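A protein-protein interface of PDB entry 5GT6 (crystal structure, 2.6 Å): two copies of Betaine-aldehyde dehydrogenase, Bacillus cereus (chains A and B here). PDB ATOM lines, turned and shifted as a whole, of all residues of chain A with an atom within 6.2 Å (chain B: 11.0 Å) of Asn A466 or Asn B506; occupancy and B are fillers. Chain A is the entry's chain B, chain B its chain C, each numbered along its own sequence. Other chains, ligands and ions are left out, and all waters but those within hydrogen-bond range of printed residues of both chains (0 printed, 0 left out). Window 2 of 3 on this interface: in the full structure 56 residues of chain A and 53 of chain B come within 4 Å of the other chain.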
ATOM      1  N   ALA A 293      17.995   3.140  33.301  1.00  0.00           N
ATOM      2  CA  ALA A 293      18.139   4.021  32.171  1.00  0.00           C
ATOM      3  C   ALA A 293      18.561   3.277  30.914  1.00  0.00           C
ATOM      4  O   ALA A 293      19.220   2.298  31.029  1.00  0.00           O
ATOM      5  CB  ALA A 293      19.207   5.035  32.478  1.00  0.00           C
ATOM      6  N   ASP A 294      18.212   3.783  29.755  1.00  0.00           N
ATOM      7  CA  ASP A 294      18.698   3.240  28.535  1.00  0.00           C
ATOM      8  C   ASP A 294      20.001   3.975  28.455  1.00  0.00           C
ATOM      9  O   ASP A 294      20.029   5.108  28.133  1.00  0.00           O
ATOM     10  CB  ASP A 294      17.846   3.594  27.352  1.00  0.00           C
ATOM     11  CG  ASP A 294      18.486   3.240  26.049  1.00  0.00           C
ATOM     12  OD1 ASP A 294      19.642   3.450  25.838  1.00  0.00           O
ATOM     13  OD2 ASP A 294      17.827   2.764  25.174  1.00  0.00           O
ATOM     14  N   GLU A 297      21.483   6.047  25.283  1.00  0.00           N
ATOM     15  CA  GLU A 297      20.875   7.384  25.136  1.00  0.00           C
ATOM     16  C   GLU A 297      21.356   8.336  26.244  1.00  0.00           C
ATOM     17  O   GLU A 297      21.567   9.501  25.980  1.00  0.00           O
ATOM     18  CB  GLU A 297      19.324   7.335  25.025  1.00  0.00           C
ATOM     19  CG  GLU A 297      18.762   7.463  23.582  1.00  0.00           C
ATOM     20  CD  GLU A 297      17.595   6.492  23.276  1.00  0.00           C
ATOM     21  OE1 GLU A 297      17.689   5.292  23.661  1.00  0.00           O
ATOM     22  OE2 GLU A 297      16.577   6.902  22.644  1.00  0.00           O
ATOM     23  N   GLY A 442      18.257  16.602  35.002  1.00  0.00           N
ATOM     24  CA  GLY A 442      18.054  15.548  34.035  1.00  0.00           C
ATOM     25  C   GLY A 442      17.874  14.264  34.793  1.00  0.00           C
ATOM     26  O   GLY A 442      18.607  14.007  35.744  1.00  0.00           O
ATOM     27  N   VAL A 443      16.907  13.454  34.380  1.00  0.00           N
ATOM     28  CA  VAL A 443      16.731  12.130  34.956  1.00  0.00           C
ATOM     29  C   VAL A 443      16.497  11.129  33.823  1.00  0.00           C
ATOM     30  O   VAL A 443      15.729  11.383  32.913  1.00  0.00           O
ATOM     31  CB  VAL A 443      15.686  12.100  36.143  1.00  0.00           C
ATOM     32  CG1 VAL A 443      14.816  13.328  36.173  1.00  0.00           C
ATOM     33  CG2 VAL A 443      14.848  10.842  36.203  1.00  0.00           C
ATOM     34  N   TRP A 444      17.229  10.019  33.896  1.00  0.00           N
ATOM     35  CA  TRP A 444      17.209   9.004  32.887  1.00  0.00           C
ATOM     36  C   TRP A 444      16.746   7.732  33.539  1.00  0.00           C
ATOM     37  O   TRP A 444      17.445   7.185  34.407  1.00  0.00           O
ATOM     38  CB  TRP A 444      18.608   8.825  32.303  1.00  0.00           C
ATOM     39  CG  TRP A 444      19.057  10.040  31.577  1.00  0.00           C
ATOM     40  CD1 TRP A 444      19.575  11.179  32.134  1.00  0.00           C
ATOM     41  CD2 TRP A 444      18.967  10.280  30.184  1.00  0.00           C
ATOM     42  NE1 TRP A 444      19.831  12.113  31.163  1.00  0.00           N
ATOM     43  CE2 TRP A 444      19.461  11.593  29.952  1.00  0.00           C
ATOM     44  CE3 TRP A 444      18.540   9.522  29.095  1.00  0.00           C
ATOM     45  CZ2 TRP A 444      19.552  12.148  28.667  1.00  0.00           C
ATOM     46  CZ3 TRP A 444      18.612  10.090  27.809  1.00  0.00           C
ATOM     47  CH2 TRP A 444      19.122  11.384  27.611  1.00  0.00           C
ATOM     48  N   THR A 445      15.567   7.273  33.129  1.00  0.00           N
ATOM     49  CA  THR A 445      15.004   6.004  33.595  1.00  0.00           C
ATOM     50  C   THR A 445      13.913   5.590  32.616  1.00  0.00           C
ATOM     51  O   THR A 445      13.255   6.429  32.062  1.00  0.00           O
ATOM     52  CB  THR A 445      14.432   6.116  35.048  1.00  0.00           C
ATOM     53  OG1 THR A 445      13.678   4.953  35.387  1.00  0.00           O
ATOM     54  CG2 THR A 445      13.517   7.313  35.217  1.00  0.00           C
ATOM     55  N   GLN A 446      13.737   4.296  32.397  1.00  0.00           N
ATOM     56  CA  GLN A 446      12.668   3.811  31.520  1.00  0.00           C
ATOM     57  C   GLN A 446      11.345   3.639  32.258  1.00  0.00           C
ATOM     58  O   GLN A 446      10.328   3.383  31.626  1.00  0.00           O
ATOM     59  CB  GLN A 446      13.091   2.486  30.827  1.00  0.00           C
ATOM     60  CG  GLN A 446      14.101   2.626  29.667  1.00  0.00           C
ATOM     61  CD  GLN A 446      13.546   3.402  28.469  1.00  0.00           C
ATOM     62  OE1 GLN A 446      14.044   4.484  28.121  1.00  0.00           O
ATOM     63  NE2 GLN A 446      12.485   2.863  27.846  1.00  0.00           N
ATOM     64  N   ASN A 447      11.354   3.724  33.572  1.00  0.00           N
ATOM     65  CA  ASN A 447      10.191   3.554  34.412  1.00  0.00           C
ATOM     66  C   ASN A 447       9.283   4.744  34.443  1.00  0.00           C
ATOM     67  O   ASN A 447       9.718   5.810  34.600  1.00  0.00           O
ATOM     68  CB  ASN A 447      10.605   3.153  35.828  1.00  0.00           C
ATOM     69  CG  ASN A 447       9.501   2.447  36.605  1.00  0.00           C
ATOM     70  OD1 ASN A 447       9.364   1.276  36.536  1.00  0.00           O
ATOM     71  ND2 ASN A 447       8.760   3.165  37.347  1.00  0.00           N
ATOM     72  N   TRP A 464      14.225  17.483  32.631  1.00  0.00           N
ATOM     73  CA  TRP A 464      14.117  16.660  31.440  1.00  0.00           C
ATOM     74  C   TRP A 464      14.143  15.180  31.831  1.00  0.00           C
ATOM     75  O   TRP A 464      15.151  14.684  32.353  1.00  0.00           O
ATOM     76  CB  TRP A 464      15.280  16.974  30.496  1.00  0.00           C
ATOM     77  CG  TRP A 464      15.371  18.389  30.015  1.00  0.00           C
ATOM     78  CD1 TRP A 464      14.614  18.997  29.059  1.00  0.00           C
ATOM     79  CD2 TRP A 464      16.329  19.349  30.429  1.00  0.00           C
ATOM     80  NE1 TRP A 464      15.044  20.309  28.856  1.00  0.00           N
ATOM     81  CE2 TRP A 464      16.095  20.534  29.702  1.00  0.00           C
ATOM     82  CE3 TRP A 464      17.388  19.325  31.341  1.00  0.00           C
ATOM     83  CZ2 TRP A 464      16.871  21.671  29.887  1.00  0.00           C
ATOM     84  CZ3 TRP A 464      18.138  20.450  31.510  1.00  0.00           C
ATOM     85  CH2 TRP A 464      17.883  21.597  30.798  1.00  0.00           C
ATOM     86  N   ILE A 465      13.040  14.481  31.582  1.00  0.00           N
ATOM     87  CA  ILE A 465      13.012  13.016  31.726  1.00  0.00           C
ATOM     88  C   ILE A 465      13.430  12.373  30.423  1.00  0.00           C
ATOM     89  O   ILE A 465      12.756  12.494  29.408  1.00  0.00           O
ATOM     90  CB  ILE A 465      11.639  12.490  32.121  1.00  0.00           C
ATOM     91  CG1 ILE A 465      11.090  13.336  33.292  1.00  0.00           C
ATOM     92  CG2 ILE A 465      11.752  10.989  32.426  1.00  0.00           C
ATOM     93  CD1 ILE A 465       9.862  12.826  33.953  1.00  0.00           C
ATOM     94  N   ASN A 466      14.564  11.694  30.468  1.00  0.00           N
ATOM     95  CA  ASN A 466      15.183  11.030  29.300  1.00  0.00           C
ATOM     96  C   ASN A 466      15.565  11.916  28.129  1.00  0.00           C
ATOM     97  O   ASN A 466      15.396  11.540  26.976  1.00  0.00           O
ATOM     98  CB  ASN A 466      14.368   9.815  28.851  1.00  0.00           C
ATOM     99  CG  ASN A 466      14.367   8.721  29.890  1.00  0.00           C
ATOM    100  OD1 ASN A 466      15.417   8.350  30.430  1.00  0.00           O
ATOM    101  ND2 ASN A 466      13.213   8.197  30.167  1.00  0.00           N
ATOM    102  N   ASP A 467      16.144  13.072  28.455  1.00  0.00           N
ATOM    103  CA  ASP A 467      16.693  14.025  27.482  1.00  0.00           C
ATOM    104  C   ASP A 467      17.432  15.121  28.234  1.00  0.00           C
ATOM    105  O   ASP A 467      17.561  15.051  29.474  1.00  0.00           O
ATOM    106  CB  ASP A 467      15.587  14.622  26.607  1.00  0.00           C
ATOM    107  CG  ASP A 467      16.023  14.777  25.159  1.00  0.00           C
ATOM    108  OD1 ASP A 467      17.138  15.298  24.970  1.00  0.00           O
ATOM    109  OD2 ASP A 467      15.261  14.431  24.228  1.00  0.00           O
ATOM    110  N   TYR A 468      17.951  16.118  27.521  1.00  0.00           N
ATOM    111  CA  TYR A 468      18.685  17.194  28.197  1.00  0.00           C
ATOM    112  C   TYR A 468      18.915  18.402  27.321  1.00  0.00           C
ATOM    113  O   TYR A 468      19.025  18.281  26.102  1.00  0.00           O
ATOM    114  CB  TYR A 468      20.041  16.685  28.744  1.00  0.00           C
ATOM    115  CG  TYR A 468      20.512  17.524  29.898  1.00  0.00           C
ATOM    116  CD1 TYR A 468      21.275  18.660  29.700  1.00  0.00           C
ATOM    117  CD2 TYR A 468      20.125  17.217  31.187  1.00  0.00           C
ATOM    118  CE1 TYR A 468      21.653  19.468  30.767  1.00  0.00           C
ATOM    119  CE2 TYR A 468      20.501  18.008  32.262  1.00  0.00           C
ATOM    120  CZ  TYR A 468      21.274  19.131  32.055  1.00  0.00           C
ATOM    121  OH  TYR A 468      21.612  19.904  33.150  1.00  0.00           O
ATOM    122  N   LEU A 470      17.016  21.066  26.419  1.00  0.00           N
ATOM    123  CA  LEU A 470      15.960  21.480  25.523  1.00  0.00           C
ATOM    124  C   LEU A 470      15.268  22.768  25.948  1.00  0.00           C
ATOM    125  O   LEU A 470      14.932  22.948  27.055  1.00  0.00           O
ATOM    126  CB  LEU A 470      14.955  20.356  25.304  1.00  0.00           C
ATOM    127  CG  LEU A 470      15.352  18.902  25.013  1.00  0.00           C
ATOM    128  CD1 LEU A 470      14.195  17.960  25.095  1.00  0.00           C
ATOM    129  CD2 LEU A 470      16.100  18.683  23.733  1.00  0.00           C
ATOM    130  N   SER B 160       5.522  19.696  20.331  1.00  0.00           N
ATOM    131  CA  SER B 160       6.109  18.727  19.429  1.00  0.00           C
ATOM    132  C   SER B 160       5.534  17.377  19.731  1.00  0.00           C
ATOM    133  O   SER B 160       5.358  17.058  20.896  1.00  0.00           O
ATOM    134  CB  SER B 160       7.609  18.713  19.747  1.00  0.00           C
ATOM    135  OG  SER B 160       8.303  17.677  19.105  1.00  0.00           O
ATOM    136  N   LYS B 161       5.292  16.536  18.736  1.00  0.00           N
ATOM    137  CA  LYS B 161       4.813  15.172  19.050  1.00  0.00           C
ATOM    138  C   LYS B 161       5.855  14.301  19.845  1.00  0.00           C
ATOM    139  O   LYS B 161       5.500  13.297  20.452  1.00  0.00           O
ATOM    140  CB  LYS B 161       4.280  14.452  17.798  1.00  0.00           C
ATOM    141  CG  LYS B 161       5.285  13.634  16.983  1.00  0.00           C
ATOM    142  CD  LYS B 161       6.261  14.512  16.181  1.00  0.00           C
ATOM    143  CE  LYS B 161       7.276  13.738  15.326  1.00  0.00           C
ATOM    144  NZ  LYS B 161       6.648  12.550  14.680  1.00  0.00           N
ATOM    145  N   ASP B 162       7.100  14.714  19.853  1.00  0.00           N
ATOM    146  CA  ASP B 162       8.179  14.022  20.502  1.00  0.00           C
ATOM    147  C   ASP B 162       8.239  14.205  22.000  1.00  0.00           C
ATOM    148  O   ASP B 162       8.935  13.493  22.680  1.00  0.00           O
ATOM    149  CB  ASP B 162       9.513  14.486  19.907  1.00  0.00           C
ATOM    150  CG  ASP B 162       9.793  13.919  18.546  1.00  0.00           C
ATOM    151  OD1 ASP B 162       9.256  12.877  18.207  1.00  0.00           O
ATOM    152  OD2 ASP B 162      10.591  14.489  17.823  1.00  0.00           O
ATOM    153  N   TYR B 163       7.541  15.197  22.502  1.00  0.00           N
ATOM    154  CA  TYR B 163       7.540  15.469  23.914  1.00  0.00           C
ATOM    155  C   TYR B 163       6.197  15.685  24.500  1.00  0.00           C
ATOM    156  O   TYR B 163       5.280  15.969  23.833  1.00  0.00           O
ATOM    157  CB  TYR B 163       8.417  16.690  24.249  1.00  0.00           C
ATOM    158  CG  TYR B 163       9.800  16.516  23.797  1.00  0.00           C
ATOM    159  CD1 TYR B 163      10.716  15.876  24.556  1.00  0.00           C
ATOM    160  CD2 TYR B 163      10.164  16.930  22.575  1.00  0.00           C
ATOM    161  CE1 TYR B 163      11.946  15.653  24.088  1.00  0.00           C
ATOM    162  CE2 TYR B 163      11.387  16.720  22.097  1.00  0.00           C
ATOM    163  CZ  TYR B 163      12.271  16.081  22.865  1.00  0.00           C
ATOM    164  OH  TYR B 163      13.507  15.886  22.393  1.00  0.00           O
ATOM    165  N   LEU B 164       6.147  15.550  25.797  1.00  0.00           N
ATOM    166  CA  LEU B 164       5.017  15.844  26.590  1.00  0.00           C
ATOM    167  C   LEU B 164       5.632  16.925  27.408  1.00  0.00           C
ATOM    168  O   LEU B 164       6.627  16.735  28.004  1.00  0.00           O
ATOM    169  CB  LEU B 164       4.548  14.691  27.444  1.00  0.00           C
ATOM    170  CG  LEU B 164       3.757  15.018  28.712  1.00  0.00           C
ATOM    171  CD1 LEU B 164       2.446  15.737  28.567  1.00  0.00           C
ATOM    172  CD2 LEU B 164       3.652  13.831  29.607  1.00  0.00           C
ATOM    173  N   ASN B 165       5.007  18.084  27.376  1.00  0.00           N
ATOM    174  CA  ASN B 165       5.454  19.273  28.046  1.00  0.00           C
ATOM    175  C   ASN B 165       4.387  19.713  28.995  1.00  0.00           C
ATOM    176  O   ASN B 165       3.247  19.915  28.591  1.00  0.00           O
ATOM    177  CB  ASN B 165       5.693  20.362  27.040  1.00  0.00           C
ATOM    178  CG  ASN B 165       6.847  20.066  26.139  1.00  0.00           C
ATOM    179  OD1 ASN B 165       6.679  19.467  25.073  1.00  0.00           O
ATOM    180  ND2 ASN B 165       8.039  20.525  26.536  1.00  0.00           N
ATOM    181  N   TYR B 166       4.760  19.849  30.258  1.00  0.00           N
ATOM    182  CA  TYR B 166       3.853  20.316  31.300  1.00  0.00           C
ATOM    183  C   TYR B 166       4.566  21.119  32.396  1.00  0.00           C
ATOM    184  O   TYR B 166       5.795  21.022  32.555  1.00  0.00           O
ATOM    185  CB  TYR B 166       3.045  19.141  31.900  1.00  0.00           C
ATOM    186  CG  TYR B 166       3.760  18.152  32.818  1.00  0.00           C
ATOM    187  CD1 TYR B 166       3.827  18.353  34.212  1.00  0.00           C
ATOM    188  CD2 TYR B 166       4.306  16.979  32.312  1.00  0.00           C
ATOM    189  CE1 TYR B 166       4.454  17.414  35.052  1.00  0.00           C
ATOM    190  CE2 TYR B 166       4.916  16.037  33.144  1.00  0.00           C
ATOM    191  CZ  TYR B 166       4.993  16.269  34.503  1.00  0.00           C
ATOM    192  OH  TYR B 166       5.584  15.338  35.282  1.00  0.00           O
ATOM    193  N   SER B 502       9.049  23.412  34.735  1.00  0.00           N
ATOM    194  CA  SER B 502       8.802  22.902  33.381  1.00  0.00           C
ATOM    195  C   SER B 502       9.416  21.516  33.180  1.00  0.00           C
ATOM    196  O   SER B 502      10.603  21.341  33.282  1.00  0.00           O
ATOM    197  CB  SER B 502       9.369  23.854  32.346  1.00  0.00           C
ATOM    198  OG  SER B 502       9.350  23.230  31.080  1.00  0.00           O
ATOM    199  N   VAL B 503       8.579  20.540  32.895  1.00  0.00           N
ATOM    200  CA  VAL B 503       8.970  19.153  32.733  1.00  0.00           C
ATOM    201  C   VAL B 503       8.851  18.803  31.243  1.00  0.00           C
ATOM    202  O   VAL B 503       7.869  19.174  30.581  1.00  0.00           O
ATOM    203  CB  VAL B 503       8.048  18.227  33.568  1.00  0.00           C
ATOM    204  CG1 VAL B 503       8.454  16.762  33.408  1.00  0.00           C
ATOM    205  CG2 VAL B 503       8.061  18.637  35.035  1.00  0.00           C
ATOM    206  N   TRP B 504       9.832  18.116  30.723  1.00  0.00           N
ATOM    207  CA  TRP B 504       9.868  17.652  29.370  1.00  0.00           C
ATOM    208  C   TRP B 504      10.027  16.166  29.438  1.00  0.00           C
ATOM    209  O   TRP B 504      10.915  15.692  30.033  1.00  0.00           O
ATOM    210  CB  TRP B 504      11.091  18.165  28.658  1.00  0.00           C
ATOM    211  CG  TRP B 504      11.197  19.576  28.402  1.00  0.00           C
ATOM    212  CD1 TRP B 504      11.299  20.546  29.296  1.00  0.00           C
ATOM    213  CD2 TRP B 504      11.298  20.183  27.144  1.00  0.00           C
ATOM    214  NE1 TRP B 504      11.416  21.726  28.706  1.00  0.00           N
ATOM    215  CE2 TRP B 504      11.444  21.535  27.361  1.00  0.00           C
ATOM    216  CE3 TRP B 504      11.276  19.713  25.839  1.00  0.00           C
ATOM    217  CZ2 TRP B 504      11.559  22.429  26.334  1.00  0.00           C
ATOM    218  CZ3 TRP B 504      11.389  20.593  24.844  1.00  0.00           C
ATOM    219  CH2 TRP B 504      11.540  21.940  25.085  1.00  0.00           C
ATOM    220  N   VAL B 505       9.139  15.440  28.817  1.00  0.00           N
ATOM    221  CA  VAL B 505       9.213  14.014  28.783  1.00  0.00           C
ATOM    222  C   VAL B 505       9.331  13.562  27.356  1.00  0.00           C
ATOM    223  O   VAL B 505       8.462  13.742  26.567  1.00  0.00           O
ATOM    224  CB  VAL B 505       7.998  13.363  29.439  1.00  0.00           C
ATOM    225  CG1 VAL B 505       8.263  11.921  29.805  1.00  0.00           C
ATOM    226  CG2 VAL B 505       7.560  14.143  30.656  1.00  0.00           C
ATOM    227  N   ASN B 506      10.472  12.979  27.060  1.00  0.00           N
ATOM    228  CA  ASN B 506      10.803  12.419  25.787  1.00  0.00           C
ATOM    229  C   ASN B 506       9.969  11.183  25.614  1.00  0.00           C
ATOM    230  O   ASN B 506      10.062  10.261  26.340  1.00  0.00           O
ATOM    231  CB  ASN B 506      12.298  12.076  25.744  1.00  0.00           C
ATOM    232  CG  ASN B 506      12.763  11.507  24.423  1.00  0.00           C
ATOM    233  OD1 ASN B 506      13.560  12.057  23.773  1.00  0.00           O
ATOM    234  ND2 ASN B 506      12.318  10.376  24.096  1.00  0.00           N
ATOM    235  N   ILE B 507       9.114  11.229  24.633  1.00  0.00           N
ATOM    236  CA  ILE B 507       8.249  10.119  24.264  1.00  0.00           C
ATOM    237  C   ILE B 507       8.461   9.716  22.811  1.00  0.00           C
ATOM    238  O   ILE B 507       7.657   9.006  22.227  1.00  0.00           O
ATOM    239  CB  ILE B 507       6.765  10.470  24.497  1.00  0.00           C
ATOM    240  CG1 ILE B 507       6.367  11.740  23.737  1.00  0.00           C
ATOM    241  CG2 ILE B 507       6.499  10.655  25.978  1.00  0.00           C
ATOM    242  CD1 ILE B 507       4.948  11.739  23.231  1.00  0.00           C
ATOM    243  N   LYS B 508       9.514  10.203  22.202  1.00  0.00           N
ATOM    244  CA  LYS B 508       9.782   9.865  20.823  1.00  0.00           C
ATOM    245  C   LYS B 508      10.309   8.457  20.795  1.00  0.00           C
ATOM    246  O   LYS B 508      10.969   8.049  21.752  1.00  0.00           O
ATOM    247  CB  LYS B 508      10.712  10.885  20.140  1.00  0.00           C
ATOM    248  CG  LYS B 508      12.186  10.589  20.063  1.00  0.00           C
ATOM    249  CD  LYS B 508      12.894  11.763  19.370  1.00  0.00           C
ATOM    250  CE  LYS B 508      13.614  12.701  20.355  1.00  0.00           C
ATOM    251  NZ  LYS B 508      14.023  14.001  19.770  1.00  0.00           N
ATOM    252  OXT LYS B 508      10.000   7.702  19.865  1.00  0.00           O
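Printed residues of chain A that touch a printed residue of chain B: Trp A464, Ile A465, Asn A466, Asp A467 and Leu A470.
Hydrophobic or aromatic side chains of chain A that line the printed part of chain B: Trp A464, Ile A465 and Leu A470.
Hydrophobic or aromatic side chains of chain B within 4 Å of the printed part of chain A: Tyr B163 and Trp B504.
Among the printed residues, 9 pairs touch across the chains.
Among the printed residues, no Asp or Glu carboxylate lies within 4 Å of a Lys or Arg side-chain nitrogen of the other chain.
No position is printed for both chains.
The backbone NH of Ile A465 sits at hydrogen-bond distance from the backbone carbonyl oxygen of Trp B504.
The backbone carbonyl oxygen (O) of Ile A465 sits at hydrogen-bond distance from the backbone NH (N) of Asn B506 (3.3 Å).
OD2 of Asp A467 is in hydrogen-bond range of OH of Tyr B163, 2.9 Å away.
The side-chain carboxylate (OD2) of Asp A467 lies close to the side-chain amide oxygen (OD1) of Asn B506 (3.0 Å).
Among the printed residues, merely in contact across the chains: Trp A464 with Trp B504, Ile A465 with Val B505, Asn A466 with Asn B506, Leu A470 with Tyr B163 and Leu A470 with Trp B504.
No residue of chain B comes within 4 Å of Val A443.
No residue of chain B comes within 4 Å of Thr A445.
Ile A465 touches three residues of chain B.
Of the printed residues of chain B, Asn A466 touches Asn B506 (3.4 Å).
Asp A467 touches two residues of chain B.
Of the printed residues of chain A, Tyr B163 touches Asp A467 (2.9 Å) and Leu A470 (3.4 Å).
Of the printed residues of chain A, Val B505 touches Ile A465.
Of chain A, only Ile A465 (3.3 Å), Asn A466 (3.4 Å) and Asp A467 (3.0 Å) come within 4 Å of Asn B506.
The nearest residue of chain A that does not touch Asn B506 is Glu A297 (5.7 Å).
The nearest printed residue of chain B that does not touch Leu A470 is Asn B506 (6.1 Å).
N of Asn A466 lies within hydrogen-bond range of O of Val A443, at 2.7 Å.
The backbone carbonyl oxygen (O) of Thr A445 lies within hydrogen-bond range of the side-chain amide nitrogen (ND2) of Asn A466 (2.6 Å).
The indole nitrogen of Trp A464 sits at hydrogen-bond distance from the backbone carbonyl oxygen of Leu A470, at 3.2 Å.
The side-chain amino group (NZ) of Lys B508 is in hydrogen-bond range of the side-chain hydroxyl (OH) of Tyr B163.
O of Leu B164 lies within hydrogen-bond range of N of Val B505, at 2.9 Å.
The backbone NH (N) of Lys B508 sits close to the side-chain amide nitrogen (ND2) of Asn B506, at 3.4 Å.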
